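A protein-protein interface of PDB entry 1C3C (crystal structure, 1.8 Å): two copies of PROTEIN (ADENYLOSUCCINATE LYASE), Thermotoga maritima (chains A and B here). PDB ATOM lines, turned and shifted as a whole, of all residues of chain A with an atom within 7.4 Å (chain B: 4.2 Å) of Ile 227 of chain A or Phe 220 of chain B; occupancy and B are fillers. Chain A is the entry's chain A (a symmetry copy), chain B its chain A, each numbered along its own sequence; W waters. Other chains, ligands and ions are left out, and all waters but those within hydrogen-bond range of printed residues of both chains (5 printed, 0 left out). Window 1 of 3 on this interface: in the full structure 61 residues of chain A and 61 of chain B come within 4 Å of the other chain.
The guanidinium group of Arg 166 of chain A is in salt-bridge range of the side-chain carboxylate of Glu 173 of chain B (2.7 Å).
The guanidinium group (NH1) of Arg 166 of chain A lies within salt-bridge range of the side-chain carboxylate (OD1) of Asp 216 of chain B (2.9 Å).
OE1 of Glu 173 of chain B lies within salt-bridge range of NH1 of Arg 217 of chain B (3.9 Å).
The backbone carbonyl oxygen of Phe 220 of chain B lies within hydrogen-bond range of the side-chain hydroxyl of Thr 224 of chain B (2.9 Å).
O of Glu 159 of chain A sits at hydrogen-bond distance from ND2 of Asn 163 of chain A (3.4 Å).
The guanidinium group of Arg 166 of chain A is in hydrogen-bond range of the side-chain amide oxygen of Asn 163 of chain A (2.9 Å).
The side-chain carboxylate of Glu 233 of chain A is in salt-bridge range of the guanidinium group of Arg 284 of chain A.
The side-chain hydroxyl of Ser 280 of chain A is in hydrogen-bond range of the guanidinium group of Arg 284 of chain A, at 3.4 Å.
OE2 of Glu 159 of chain A touches CB of Asp 216 of chain B (3.5 Å).
NE of Arg 166 of chain A touches CD1 of Phe 220 of chain B, at 3.9 Å.
Ile 227 of chain A touches Phe 220 of chain B.
CG1 of Ile 227 of chain A touches CD2 of Leu 291 of chain B, at 3.5 Å.
Leu 291 of chain B touches Ala 230 of chain A (O to CB, 3.9 Å).
Leu 291 of chain B touches Arg 284 of chain A (CD1 to CB, 3.8 Å).
Of chain B, only Phe 220 (3.6 Å) and Leu 291 (3.5 Å) come within 4 Å of Ile 227 of chain A.
Of the printed residues of chain A, Asp 216 of chain B touches Glu 159 (3.5 Å) and Arg 166 (2.9 Å).
Printed residues of chain A within 4 Å of Leu 291 of chain B: Ile 227 (3.5 Å), Ala 230 (3.9 Å) and Arg 284 (3.8 Å).
Printed residues of chain B within 4 Å of Ala 230 of chain A: Leu 291.
Of the printed residues of chain B, Arg 284 of chain A touches Leu 291 (3.8 Å).
Of the printed residues of chain B, Arg 166 of chain A touches Glu 173 (2.7 Å), Asp 216 (2.9 Å) and Phe 220 (3.9 Å).
The nearest residue of chain B that does not touch Ile 227 of chain A is Ser 223 of chain B (4.1 Å).
The nearest residue of chain A that does not touch Phe 220 of chain B is Phe 220 of chain A (4.4 Å).
Hydrophobic or aromatic side chains of chain B within 4 Å of the printed part of chain A: Phe 220 and Leu 291.
Hydrophobic or aromatic side chains of chain A within 4 Å of the printed part of chain B: Ile 227 and Ala 230.
Among the printed residues, 8 pairs touch across the chains.
5 positions are printed for both chains.
Of the 8 pairs that touch across the chains among the printed residues, none has its exchanged pair printed and touching as well.
Water W1 lies within hydrogen-bond range of the guanidinium group (NH2) of Arg 169 of chain A and the side-chain carboxylate (OE2) of Glu 173 of chain B.
Water W3 bridges the backbone carbonyl oxygen of Leu 291 of chain B and the side-chain carboxylate of Glu 233 of chain A.
Water W4 bridges OD2 of Asp 216 of chain B (2.7 Å) and OE2 of Glu 159 of chain A (2.8 Å).
Water W2 lies within hydrogen-bond range of the side-chain hydroxyl (OG) of Ser 223 of chain A and the backbone carbonyl oxygen (O) of Ser 223 of chain B.
Water W5 lies within hydrogen-bond range of OG of Ser 223 of chain B (2.8 Å) and O of Ser 223 of chain A (3.0 Å).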
ATOM      1  N   GLU A 159      13.393 -13.332  12.151  1.00  0.00           N
ATOM      2  CA  GLU A 159      14.031 -12.264  11.352  1.00  0.00           C
ATOM      3  C   GLU A 159      15.550 -12.410  11.300  1.00  0.00           C
ATOM      4  O   GLU A 159      16.136 -12.321  10.197  1.00  0.00           O
ATOM      5  CB  GLU A 159      13.678 -10.900  11.959  1.00  0.00           C
ATOM      6  CG  GLU A 159      14.168  -9.746  11.063  1.00  0.00           C
ATOM      7  CD  GLU A 159      13.494  -8.415  11.341  1.00  0.00           C
ATOM      8  OE1 GLU A 159      12.759  -8.318  12.352  1.00  0.00           O
ATOM      9  OE2 GLU A 159      13.651  -7.413  10.544  1.00  0.00           O
ATOM     10  N   MET A 160      16.187 -12.660  12.457  1.00  0.00           N
ATOM     11  CA  MET A 160      17.632 -12.803  12.491  1.00  0.00           C
ATOM     12  C   MET A 160      18.056 -14.067  11.745  1.00  0.00           C
ATOM     13  O   MET A 160      19.142 -14.029  11.117  1.00  0.00           O
ATOM     14  CB  MET A 160      18.248 -12.708  13.907  1.00  0.00           C
ATOM     15  CG  MET A 160      18.037 -11.313  14.546  1.00  0.00           C
ATOM     16  SD  MET A 160      18.908  -9.947  13.540  1.00  0.00           S
ATOM     17  CE  MET A 160      17.487  -8.910  13.415  1.00  0.00           C
ATOM     18  N   ASN A 163      18.206 -13.081   8.281  1.00  0.00           N
ATOM     19  CA  ASN A 163      19.407 -12.243   8.083  1.00  0.00           C
ATOM     20  C   ASN A 163      20.675 -13.087   8.047  1.00  0.00           C
ATOM     21  O   ASN A 163      21.604 -12.753   7.302  1.00  0.00           O
ATOM     22  CB  ASN A 163      19.460 -11.184   9.192  1.00  0.00           C
ATOM     23  CG  ASN A 163      18.469 -10.052   8.898  1.00  0.00           C
ATOM     24  OD1 ASN A 163      18.276  -9.752   7.702  1.00  0.00           O
ATOM     25  ND2 ASN A 163      17.951  -9.461   9.964  1.00  0.00           N
ATOM     26  N   ARG A 166      20.751 -14.119   4.463  1.00  0.00           N
ATOM     27  CA  ARG A 166      21.068 -12.961   3.613  1.00  0.00           C
ATOM     28  C   ARG A 166      22.545 -12.594   3.725  1.00  0.00           C
ATOM     29  O   ARG A 166      23.178 -12.221   2.724  1.00  0.00           O
ATOM     30  CB  ARG A 166      20.217 -11.733   4.010  1.00  0.00           C
ATOM     31  CG  ARG A 166      18.745 -11.884   3.630  1.00  0.00           C
ATOM     32  CD  ARG A 166      17.908 -10.862   4.439  1.00  0.00           C
ATOM     33  NE  ARG A 166      16.466 -11.073   4.126  1.00  0.00           N
ATOM     34  CZ  ARG A 166      15.539 -10.637   4.992  1.00  0.00           C
ATOM     35  NH1 ARG A 166      15.879 -10.003   6.124  1.00  0.00           N
ATOM     36  NH2 ARG A 166      14.280 -10.872   4.622  1.00  0.00           N
ATOM     37  N   ARG A 169      24.653 -14.908   1.646  1.00  0.00           N
ATOM     38  CA  ARG A 169      24.610 -14.544   0.242  1.00  0.00           C
ATOM     39  C   ARG A 169      25.438 -13.291  -0.046  1.00  0.00           C
ATOM     40  O   ARG A 169      26.095 -13.215  -1.089  1.00  0.00           O
ATOM     41  CB  ARG A 169      23.145 -14.388  -0.236  1.00  0.00           C
ATOM     42  CG  ARG A 169      22.593 -15.814  -0.346  1.00  0.00           C
ATOM     43  CD  ARG A 169      21.240 -15.951  -0.982  1.00  0.00           C
ATOM     44  NE  ARG A 169      20.193 -15.501  -0.066  1.00  0.00           N
ATOM     45  CZ  ARG A 169      19.561 -16.318   0.813  1.00  0.00           C
ATOM     46  NH1 ARG A 169      19.859 -17.616   0.871  1.00  0.00           N
ATOM     47  NH2 ARG A 169      18.640 -15.762   1.613  1.00  0.00           N
ATOM     48  N   PHE A 220      25.060  -4.433  -2.991  1.00  0.00           N
ATOM     49  CA  PHE A 220      24.262  -5.551  -2.451  1.00  0.00           C
ATOM     50  C   PHE A 220      24.670  -5.896  -1.024  1.00  0.00           C
ATOM     51  O   PHE A 220      23.802  -6.094  -0.138  1.00  0.00           O
ATOM     52  CB  PHE A 220      24.469  -6.765  -3.403  1.00  0.00           C
ATOM     53  CG  PHE A 220      23.625  -7.922  -2.923  1.00  0.00           C
ATOM     54  CD1 PHE A 220      22.319  -7.998  -3.389  1.00  0.00           C
ATOM     55  CD2 PHE A 220      24.135  -8.843  -2.039  1.00  0.00           C
ATOM     56  CE1 PHE A 220      21.516  -9.086  -2.954  1.00  0.00           C
ATOM     57  CE2 PHE A 220      23.332  -9.896  -1.593  1.00  0.00           C
ATOM     58  CZ  PHE A 220      22.035  -9.978  -2.061  1.00  0.00           C
ATOM     59  N   TYR A 221      25.973  -5.966  -0.786  1.00  0.00           N
ATOM     60  CA  TYR A 221      26.477  -6.261   0.589  1.00  0.00           C
ATOM     61  C   TYR A 221      26.012  -5.203   1.563  1.00  0.00           C
ATOM     62  O   TYR A 221      25.528  -5.497   2.668  1.00  0.00           O
ATOM     63  CB  TYR A 221      27.998  -6.286   0.523  1.00  0.00           C
ATOM     64  CG  TYR A 221      28.808  -6.619   1.759  1.00  0.00           C
ATOM     65  CD1 TYR A 221      29.300  -7.920   1.940  1.00  0.00           C
ATOM     66  CD2 TYR A 221      29.151  -5.607   2.647  1.00  0.00           C
ATOM     67  CE1 TYR A 221      30.080  -8.180   3.084  1.00  0.00           C
ATOM     68  CE2 TYR A 221      29.983  -5.859   3.746  1.00  0.00           C
ATOM     69  CZ  TYR A 221      30.415  -7.155   3.946  1.00  0.00           C
ATOM     70  OH  TYR A 221      31.246  -7.373   5.001  1.00  0.00           O
ATOM     71  N   LEU A 222      26.155  -3.921   1.208  1.00  0.00           N
ATOM     72  CA  LEU A 222      25.818  -2.861   2.181  1.00  0.00           C
ATOM     73  C   LEU A 222      24.310  -2.738   2.365  1.00  0.00           C
ATOM     74  O   LEU A 222      23.809  -2.441   3.448  1.00  0.00           O
ATOM     75  CB  LEU A 222      26.435  -1.504   1.731  1.00  0.00           C
ATOM     76  CG  LEU A 222      27.984  -1.509   1.846  1.00  0.00           C
ATOM     77  CD1 LEU A 222      28.620  -0.433   1.004  1.00  0.00           C
ATOM     78  CD2 LEU A 222      28.434  -1.458   3.315  1.00  0.00           C
ATOM     79  N   SER A 223      23.522  -3.000   1.311  1.00  0.00           N
ATOM     80  CA  SER A 223      22.063  -3.027   1.426  1.00  0.00           C
ATOM     81  C   SER A 223      21.629  -4.117   2.407  1.00  0.00           C
ATOM     82  O   SER A 223      20.746  -3.921   3.252  1.00  0.00           O
ATOM     83  CB  SER A 223      21.396  -3.360   0.056  1.00  0.00           C
ATOM     84  OG  SER A 223      21.576  -2.203  -0.771  1.00  0.00           O
ATOM     85  N   THR A 224      22.283  -5.276   2.272  1.00  0.00           N
ATOM     86  CA  THR A 224      22.062  -6.366   3.199  1.00  0.00           C
ATOM     87  C   THR A 224      22.345  -5.991   4.650  1.00  0.00           C
ATOM     88  O   THR A 224      21.538  -6.264   5.547  1.00  0.00           O
ATOM     89  CB  THR A 224      22.949  -7.592   2.805  1.00  0.00           C
ATOM     90  OG1 THR A 224      22.457  -8.005   1.519  1.00  0.00           O
ATOM     91  CG2 THR A 224      22.714  -8.714   3.807  1.00  0.00           C
ATOM     92  N   LEU A 225      23.496  -5.363   4.900  1.00  0.00           N
ATOM     93  CA  LEU A 225      23.842  -4.895   6.246  1.00  0.00           C
ATOM     94  C   LEU A 225      22.787  -3.944   6.802  1.00  0.00           C
ATOM     95  O   LEU A 225      22.517  -4.014   8.006  1.00  0.00           O
ATOM     96  CB  LEU A 225      25.215  -4.216   6.232  1.00  0.00           C
ATOM     97  CG  LEU A 225      26.445  -5.083   6.430  1.00  0.00           C
ATOM     98  CD1 LEU A 225      26.334  -6.540   6.055  1.00  0.00           C
ATOM     99  CD2 LEU A 225      27.812  -4.475   6.337  1.00  0.00           C
ATOM    100  N   ALA A 226      22.278  -3.047   5.961  1.00  0.00           N
ATOM    101  CA  ALA A 226      21.293  -2.078   6.472  1.00  0.00           C
ATOM    102  C   ALA A 226      19.986  -2.768   6.884  1.00  0.00           C
ATOM    103  O   ALA A 226      19.301  -2.342   7.846  1.00  0.00           O
ATOM    104  CB  ALA A 226      21.028  -1.033   5.391  1.00  0.00           C
ATOM    105  N   ILE A 227      19.612  -3.814   6.154  1.00  0.00           N
ATOM    106  CA  ILE A 227      18.419  -4.604   6.525  1.00  0.00           C
ATOM    107  C   ILE A 227      18.662  -5.322   7.841  1.00  0.00           C
ATOM    108  O   ILE A 227      17.724  -5.401   8.669  1.00  0.00           O
ATOM    109  CB  ILE A 227      18.048  -5.592   5.382  1.00  0.00           C
ATOM    110  CG1 ILE A 227      17.581  -4.730   4.175  1.00  0.00           C
ATOM    111  CG2 ILE A 227      16.942  -6.564   5.815  1.00  0.00           C
ATOM    112  CD1 ILE A 227      17.441  -5.560   2.887  1.00  0.00           C
ATOM    113  N   VAL A 228      19.844  -5.892   8.053  1.00  0.00           N
ATOM    114  CA  VAL A 228      20.117  -6.499   9.368  1.00  0.00           C
ATOM    115  C   VAL A 228      19.954  -5.471  10.492  1.00  0.00           C
ATOM    116  O   VAL A 228      19.305  -5.724  11.525  1.00  0.00           O
ATOM    117  CB  VAL A 228      21.514  -7.135   9.414  1.00  0.00           C
ATOM    118  CG1 VAL A 228      21.712  -7.880  10.757  1.00  0.00           C
ATOM    119  CG2 VAL A 228      21.708  -8.139   8.260  1.00  0.00           C
ATOM    120  N   ALA A 229      20.558  -4.288  10.291  1.00  0.00           N
ATOM    121  CA  ALA A 229      20.440  -3.210  11.245  1.00  0.00           C
ATOM    122  C   ALA A 229      18.992  -2.847  11.536  1.00  0.00           C
ATOM    123  O   ALA A 229      18.686  -2.516  12.699  1.00  0.00           O
ATOM    124  CB  ALA A 229      21.199  -1.985  10.700  1.00  0.00           C
ATOM    125  N   ALA A 230      18.119  -2.737  10.534  1.00  0.00           N
ATOM    126  CA  ALA A 230      16.730  -2.321  10.768  1.00  0.00           C
ATOM    127  C   ALA A 230      16.006  -3.395  11.590  1.00  0.00           C
ATOM    128  O   ALA A 230      15.065  -3.081  12.332  1.00  0.00           O
ATOM    129  CB  ALA A 230      16.011  -2.125   9.422  1.00  0.00           C
ATOM    130  N   GLY A 231      16.372  -4.643  11.386  1.00  0.00           N
ATOM    131  CA  GLY A 231      15.822  -5.719  12.263  1.00  0.00           C
ATOM    132  C   GLY A 231      16.227  -5.498  13.722  1.00  0.00           C
ATOM    133  O   GLY A 231      15.392  -5.734  14.608  1.00  0.00           O
ATOM    134  N   ILE A 232      17.472  -5.126  13.992  1.00  0.00           N
ATOM    135  CA  ILE A 232      17.910  -4.837  15.347  1.00  0.00           C
ATOM    136  C   ILE A 232      17.150  -3.595  15.823  1.00  0.00           C
ATOM    137  O   ILE A 232      16.726  -3.574  16.991  1.00  0.00           O
ATOM    138  CB  ILE A 232      19.431  -4.628  15.430  1.00  0.00           C
ATOM    139  CG1 ILE A 232      20.109  -5.974  15.083  1.00  0.00           C
ATOM    140  CG2 ILE A 232      19.855  -4.145  16.830  1.00  0.00           C
ATOM    141  CD1 ILE A 232      21.621  -5.915  14.843  1.00  0.00           C
ATOM    142  N   GLU A 233      16.954  -2.590  14.951  1.00  0.00           N
ATOM    143  CA  GLU A 233      16.174  -1.414  15.363  1.00  0.00           C
ATOM    144  C   GLU A 233      14.764  -1.796  15.805  1.00  0.00           C
ATOM    145  O   GLU A 233      14.235  -1.211  16.768  1.00  0.00           O
ATOM    146  CB  GLU A 233      16.157  -0.447  14.152  1.00  0.00           C
ATOM    147  CG  GLU A 233      15.419   0.876  14.372  1.00  0.00           C
ATOM    148  CD  GLU A 233      15.254   1.600  13.032  1.00  0.00           C
ATOM    149  OE1 GLU A 233      15.783   1.153  11.956  1.00  0.00           O
ATOM    150  OE2 GLU A 233      14.572   2.644  13.053  1.00  0.00           O
ATOM    151  N   SER A 280      21.183   2.354  13.653  1.00  0.00           N
ATOM    152  CA  SER A 280      20.485   1.861  12.458  1.00  0.00           C
ATOM    153  C   SER A 280      20.227   2.964  11.446  1.00  0.00           C
ATOM    154  O   SER A 280      20.256   2.699  10.232  1.00  0.00           O
ATOM    155  CB  SER A 280      19.124   1.263  12.872  1.00  0.00           C
ATOM    156  OG  SER A 280      18.519   0.707  11.700  1.00  0.00           O
ATOM    157  N   MET A 283      23.378   3.119   9.398  1.00  0.00           N
ATOM    158  CA  MET A 283      23.543   1.959   8.531  1.00  0.00           C
ATOM    159  C   MET A 283      22.699   2.135   7.280  1.00  0.00           C
ATOM    160  O   MET A 283      23.142   1.909   6.130  1.00  0.00           O
ATOM    161  CB  MET A 283      23.070   0.710   9.290  1.00  0.00           C
ATOM    162  CG  MET A 283      23.965   0.290  10.441  1.00  0.00           C
ATOM    163  SD  MET A 283      25.721  -0.128   9.854  1.00  0.00           S
ATOM    164  CE  MET A 283      25.306  -1.476   8.630  1.00  0.00           C
ATOM    165  N   ARG A 284      21.467   2.616   7.457  1.00  0.00           N
ATOM    166  CA  ARG A 284      20.664   2.842   6.225  1.00  0.00           C
ATOM    167  C   ARG A 284      21.166   4.043   5.482  1.00  0.00           C
ATOM    168  O   ARG A 284      21.086   4.065   4.224  1.00  0.00           O
ATOM    169  CB  ARG A 284      19.192   2.822   6.535  1.00  0.00           C
ATOM    170  CG  ARG A 284      18.621   4.036   7.162  1.00  0.00           C
ATOM    171  CD  ARG A 284      17.053   3.922   7.087  1.00  0.00           C
ATOM    172  NE  ARG A 284      16.537   4.363   8.371  1.00  0.00           N
ATOM    173  CZ  ARG A 284      16.270   3.577   9.402  1.00  0.00           C
ATOM    174  NH1 ARG A 284      16.450   2.254   9.426  1.00  0.00           N
ATOM    175  NH2 ARG A 284      15.763   4.159  10.494  1.00  0.00           N
ATOM    176  N   VAL A 287      23.455   3.220   2.417  1.00  0.00           N
ATOM    177  CA  VAL A 287      22.971   2.515   1.229  1.00  0.00           C
ATOM    178  C   VAL A 287      22.967   3.433   0.009  1.00  0.00           C
ATOM    179  O   VAL A 287      23.493   3.054  -1.058  1.00  0.00           O
ATOM    180  CB  VAL A 287      21.555   1.951   1.483  1.00  0.00           C
ATOM    181  CG1 VAL A 287      21.039   1.278   0.198  1.00  0.00           C
ATOM    182  CG2 VAL A 287      21.579   0.965   2.652  1.00  0.00           C
ATOM    183  N   LEU A 319      27.734  -2.236  12.425  1.00  0.00           N
ATOM    184  CA  LEU A 319      26.816  -3.383  12.568  1.00  0.00           C
ATOM    185  C   LEU A 319      27.341  -4.398  13.577  1.00  0.00           C
ATOM    186  O   LEU A 319      26.551  -4.994  14.302  1.00  0.00           O
ATOM    187  CB  LEU A 319      26.625  -4.070  11.215  1.00  0.00           C
ATOM    188  CG  LEU A 319      25.340  -4.820  10.912  1.00  0.00           C
ATOM    189  CD1 LEU A 319      25.439  -5.989   9.934  1.00  0.00           C
ATOM    190  CD2 LEU A 319      24.210  -4.915  11.870  1.00  0.00           C
ATOM    191  N   ALA B 170      14.769 -12.344  -4.550  1.00  0.00           N
ATOM    192  CA  ALA B 170      13.779 -11.375  -4.042  1.00  0.00           C
ATOM    193  C   ALA B 170      12.361 -11.899  -4.216  1.00  0.00           C
ATOM    194  O   ALA B 170      11.526 -11.698  -3.334  1.00  0.00           O
ATOM    195  CB  ALA B 170      13.975 -10.057  -4.800  1.00  0.00           C
ATOM    196  N   GLU B 173      11.784 -14.239  -1.431  1.00  0.00           N
ATOM    197  CA  GLU B 173      11.617 -13.537  -0.159  1.00  0.00           C
ATOM    198  C   GLU B 173      10.185 -13.014   0.046  1.00  0.00           C
ATOM    199  O   GLU B 173       9.758 -12.915   1.211  1.00  0.00           O
ATOM    200  CB  GLU B 173      12.570 -12.319  -0.066  1.00  0.00           C
ATOM    201  CG  GLU B 173      14.013 -12.725   0.165  1.00  0.00           C
ATOM    202  CD  GLU B 173      14.478 -12.449   1.598  1.00  0.00           C
ATOM    203  OE1 GLU B 173      13.571 -12.125   2.391  1.00  0.00           O
ATOM    204  OE2 GLU B 173      15.679 -12.528   1.894  1.00  0.00           O
ATOM    205  N   ASP B 216      10.881  -6.585   6.649  1.00  0.00           N
ATOM    206  CA  ASP B 216      12.232  -6.738   6.067  1.00  0.00           C
ATOM    207  C   ASP B 216      12.130  -7.482   4.736  1.00  0.00           C
ATOM    208  O   ASP B 216      13.025  -7.299   3.911  1.00  0.00           O
ATOM    209  CB  ASP B 216      13.146  -7.483   7.047  1.00  0.00           C
ATOM    210  CG  ASP B 216      12.606  -8.849   7.446  1.00  0.00           C
ATOM    211  OD1 ASP B 216      13.189  -9.921   7.136  1.00  0.00           O
ATOM    212  OD2 ASP B 216      11.530  -8.924   8.096  1.00  0.00           O
ATOM    213  N   ARG B 217      11.101  -8.338   4.515  1.00  0.00           N
ATOM    214  CA  ARG B 217      10.999  -8.975   3.205  1.00  0.00           C
ATOM    215  C   ARG B 217      10.801  -7.936   2.101  1.00  0.00           C
ATOM    216  O   ARG B 217      11.426  -8.031   1.037  1.00  0.00           O
ATOM    217  CB  ARG B 217       9.754  -9.903   3.217  1.00  0.00           C
ATOM    218  CG  ARG B 217       9.897 -11.032   4.266  1.00  0.00           C
ATOM    219  CD  ARG B 217       8.685 -12.009   4.135  1.00  0.00           C
ATOM    220  NE  ARG B 217       8.841 -13.143   5.057  1.00  0.00           N
ATOM    221  CZ  ARG B 217       9.725 -14.135   4.872  1.00  0.00           C
ATOM    222  NH1 ARG B 217      10.531 -14.200   3.796  1.00  0.00           N
ATOM    223  NH2 ARG B 217       9.815 -15.142   5.775  1.00  0.00           N
ATOM    224  N   HIS B 218       9.854  -7.011   2.335  1.00  0.00           N
ATOM    225  CA  HIS B 218       9.588  -5.996   1.290  1.00  0.00           C
ATOM    226  C   HIS B 218      10.808  -5.102   1.088  1.00  0.00           C
ATOM    227  O   HIS B 218      11.035  -4.682  -0.074  1.00  0.00           O
ATOM    228  CB  HIS B 218       8.353  -5.149   1.701  1.00  0.00           C
ATOM    229  CG  HIS B 218       7.240  -6.051   2.165  1.00  0.00           C
ATOM    230  ND1 HIS B 218       7.220  -6.617   3.420  1.00  0.00           N
ATOM    231  CD2 HIS B 218       6.103  -6.478   1.531  1.00  0.00           C
ATOM    232  CE1 HIS B 218       6.110  -7.361   3.547  1.00  0.00           C
ATOM    233  NE2 HIS B 218       5.415  -7.290   2.419  1.00  0.00           N
ATOM    234  N   ALA B 219      11.539  -4.790   2.158  1.00  0.00           N
ATOM    235  CA  ALA B 219      12.734  -3.932   2.003  1.00  0.00           C
ATOM    236  C   ALA B 219      13.813  -4.669   1.213  1.00  0.00           C
ATOM    237  O   ALA B 219      14.521  -4.086   0.397  1.00  0.00           O
ATOM    238  CB  ALA B 219      13.339  -3.587   3.380  1.00  0.00           C
ATOM    239  N   PHE B 220      13.986  -5.972   1.435  1.00  0.00           N
ATOM    240  CA  PHE B 220      14.933  -6.747   0.610  1.00  0.00           C
ATOM    241  C   PHE B 220      14.550  -6.717  -0.864  1.00  0.00           C
ATOM    242  O   PHE B 220      15.417  -6.512  -1.749  1.00  0.00           O
ATOM    243  CB  PHE B 220      14.936  -8.203   1.160  1.00  0.00           C
ATOM    244  CG  PHE B 220      15.937  -9.025   0.382  1.00  0.00           C
ATOM    245  CD1 PHE B 220      17.249  -9.034   0.836  1.00  0.00           C
ATOM    246  CD2 PHE B 220      15.553  -9.714  -0.744  1.00  0.00           C
ATOM    247  CE1 PHE B 220      18.199  -9.810   0.121  1.00  0.00           C
ATOM    248  CE2 PHE B 220      16.497 -10.455  -1.460  1.00  0.00           C
ATOM    249  CZ  PHE B 220      17.803 -10.471  -1.007  1.00  0.00           C
ATOM    250  N   TYR B 221      13.268  -6.913  -1.143  1.00  0.00           N
ATOM    251  CA  TYR B 221      12.783  -6.867  -2.555  1.00  0.00           C
ATOM    252  C   TYR B 221      13.059  -5.512  -3.165  1.00  0.00           C
ATOM    253  O   TYR B 221      13.556  -5.391  -4.297  1.00  0.00           O
ATOM    254  CB  TYR B 221      11.286  -7.142  -2.534  1.00  0.00           C
ATOM    255  CG  TYR B 221      10.508  -7.219  -3.832  1.00  0.00           C
ATOM    256  CD1 TYR B 221      10.217  -8.469  -4.397  1.00  0.00           C
ATOM    257  CD2 TYR B 221       9.994  -6.056  -4.392  1.00  0.00           C
ATOM    258  CE1 TYR B 221       9.461  -8.499  -5.585  1.00  0.00           C
ATOM    259  CE2 TYR B 221       9.185  -6.100  -5.536  1.00  0.00           C
ATOM    260  CZ  TYR B 221       8.952  -7.331  -6.116  1.00  0.00           C
ATOM    261  OH  TYR B 221       8.140  -7.356  -7.207  1.00  0.00           O
ATOM    262  N   LEU B 222      12.729  -4.428  -2.455  1.00  0.00           N
ATOM    263  CA  LEU B 222      12.877  -3.090  -3.067  1.00  0.00           C
ATOM    264  C   LEU B 222      14.344  -2.690  -3.171  1.00  0.00           C
ATOM    265  O   LEU B 222      14.768  -2.016  -4.108  1.00  0.00           O
ATOM    266  CB  LEU B 222      12.070  -2.036  -2.253  1.00  0.00           C
ATOM    267  CG  LEU B 222      10.538  -2.245  -2.400  1.00  0.00           C
ATOM    268  CD1 LEU B 222       9.764  -1.573  -1.295  1.00  0.00           C
ATOM    269  CD2 LEU B 222      10.051  -1.835  -3.800  1.00  0.00           C
ATOM    270  N   SER B 223      15.187  -3.125  -2.223  1.00  0.00           N
ATOM    271  CA  SER B 223      16.630  -2.893  -2.307  1.00  0.00           C
ATOM    272  C   SER B 223      17.203  -3.569  -3.554  1.00  0.00           C
ATOM    273  O   SER B 223      18.026  -3.001  -4.283  1.00  0.00           O
ATOM    274  CB  SER B 223      17.371  -3.506  -1.079  1.00  0.00           C
ATOM    275  OG  SER B 223      17.035  -2.683   0.046  1.00  0.00           O
ATOM    276  N   THR B 224      16.737  -4.802  -3.779  1.00  0.00           N
ATOM    277  CA  THR B 224      17.101  -5.526  -4.978  1.00  0.00           C
ATOM    278  C   THR B 224      16.731  -4.791  -6.263  1.00  0.00           C
ATOM    279  O   THR B 224      17.549  -4.662  -7.181  1.00  0.00           O
ATOM    280  CB  THR B 224      16.421  -6.934  -4.981  1.00  0.00           C
ATOM    281  OG1 THR B 224      17.000  -7.625  -3.862  1.00  0.00           O
ATOM    282  CG2 THR B 224      16.802  -7.664  -6.262  1.00  0.00           C
ATOM    283  N   LEU B 291      13.158   0.735   4.205  1.00  0.00           N
ATOM    284  CA  LEU B 291      13.904   0.265   5.369  1.00  0.00           C
ATOM    285  C   LEU B 291      13.328   0.846   6.670  1.00  0.00           C
ATOM    286  O   LEU B 291      13.324   0.176   7.708  1.00  0.00           O
ATOM    287  CB  LEU B 291      15.389   0.731   5.289  1.00  0.00           C
ATOM    288  CG  LEU B 291      16.165  -0.062   4.183  1.00  0.00           C
ATOM    289  CD1 LEU B 291      17.431   0.745   3.892  1.00  0.00           C
ATOM    290  CD2 LEU B 291      16.513  -1.410   4.774  1.00  0.00           C
HETATM  291  O   HOH W   1      17.579 -13.728   0.390  1.00  0.00           O
HETATM  292  O   HOH W   2      19.519  -1.170  -2.441  1.00  0.00           O
HETATM  293  O   HOH W   3      13.173   0.498  10.376  1.00  0.00           O
HETATM  294  O   HOH W   4      10.907  -7.258  10.151  1.00  0.00           O
HETATM  295  O   HOH W   5      18.948  -1.882   1.992  1.00  0.00           O
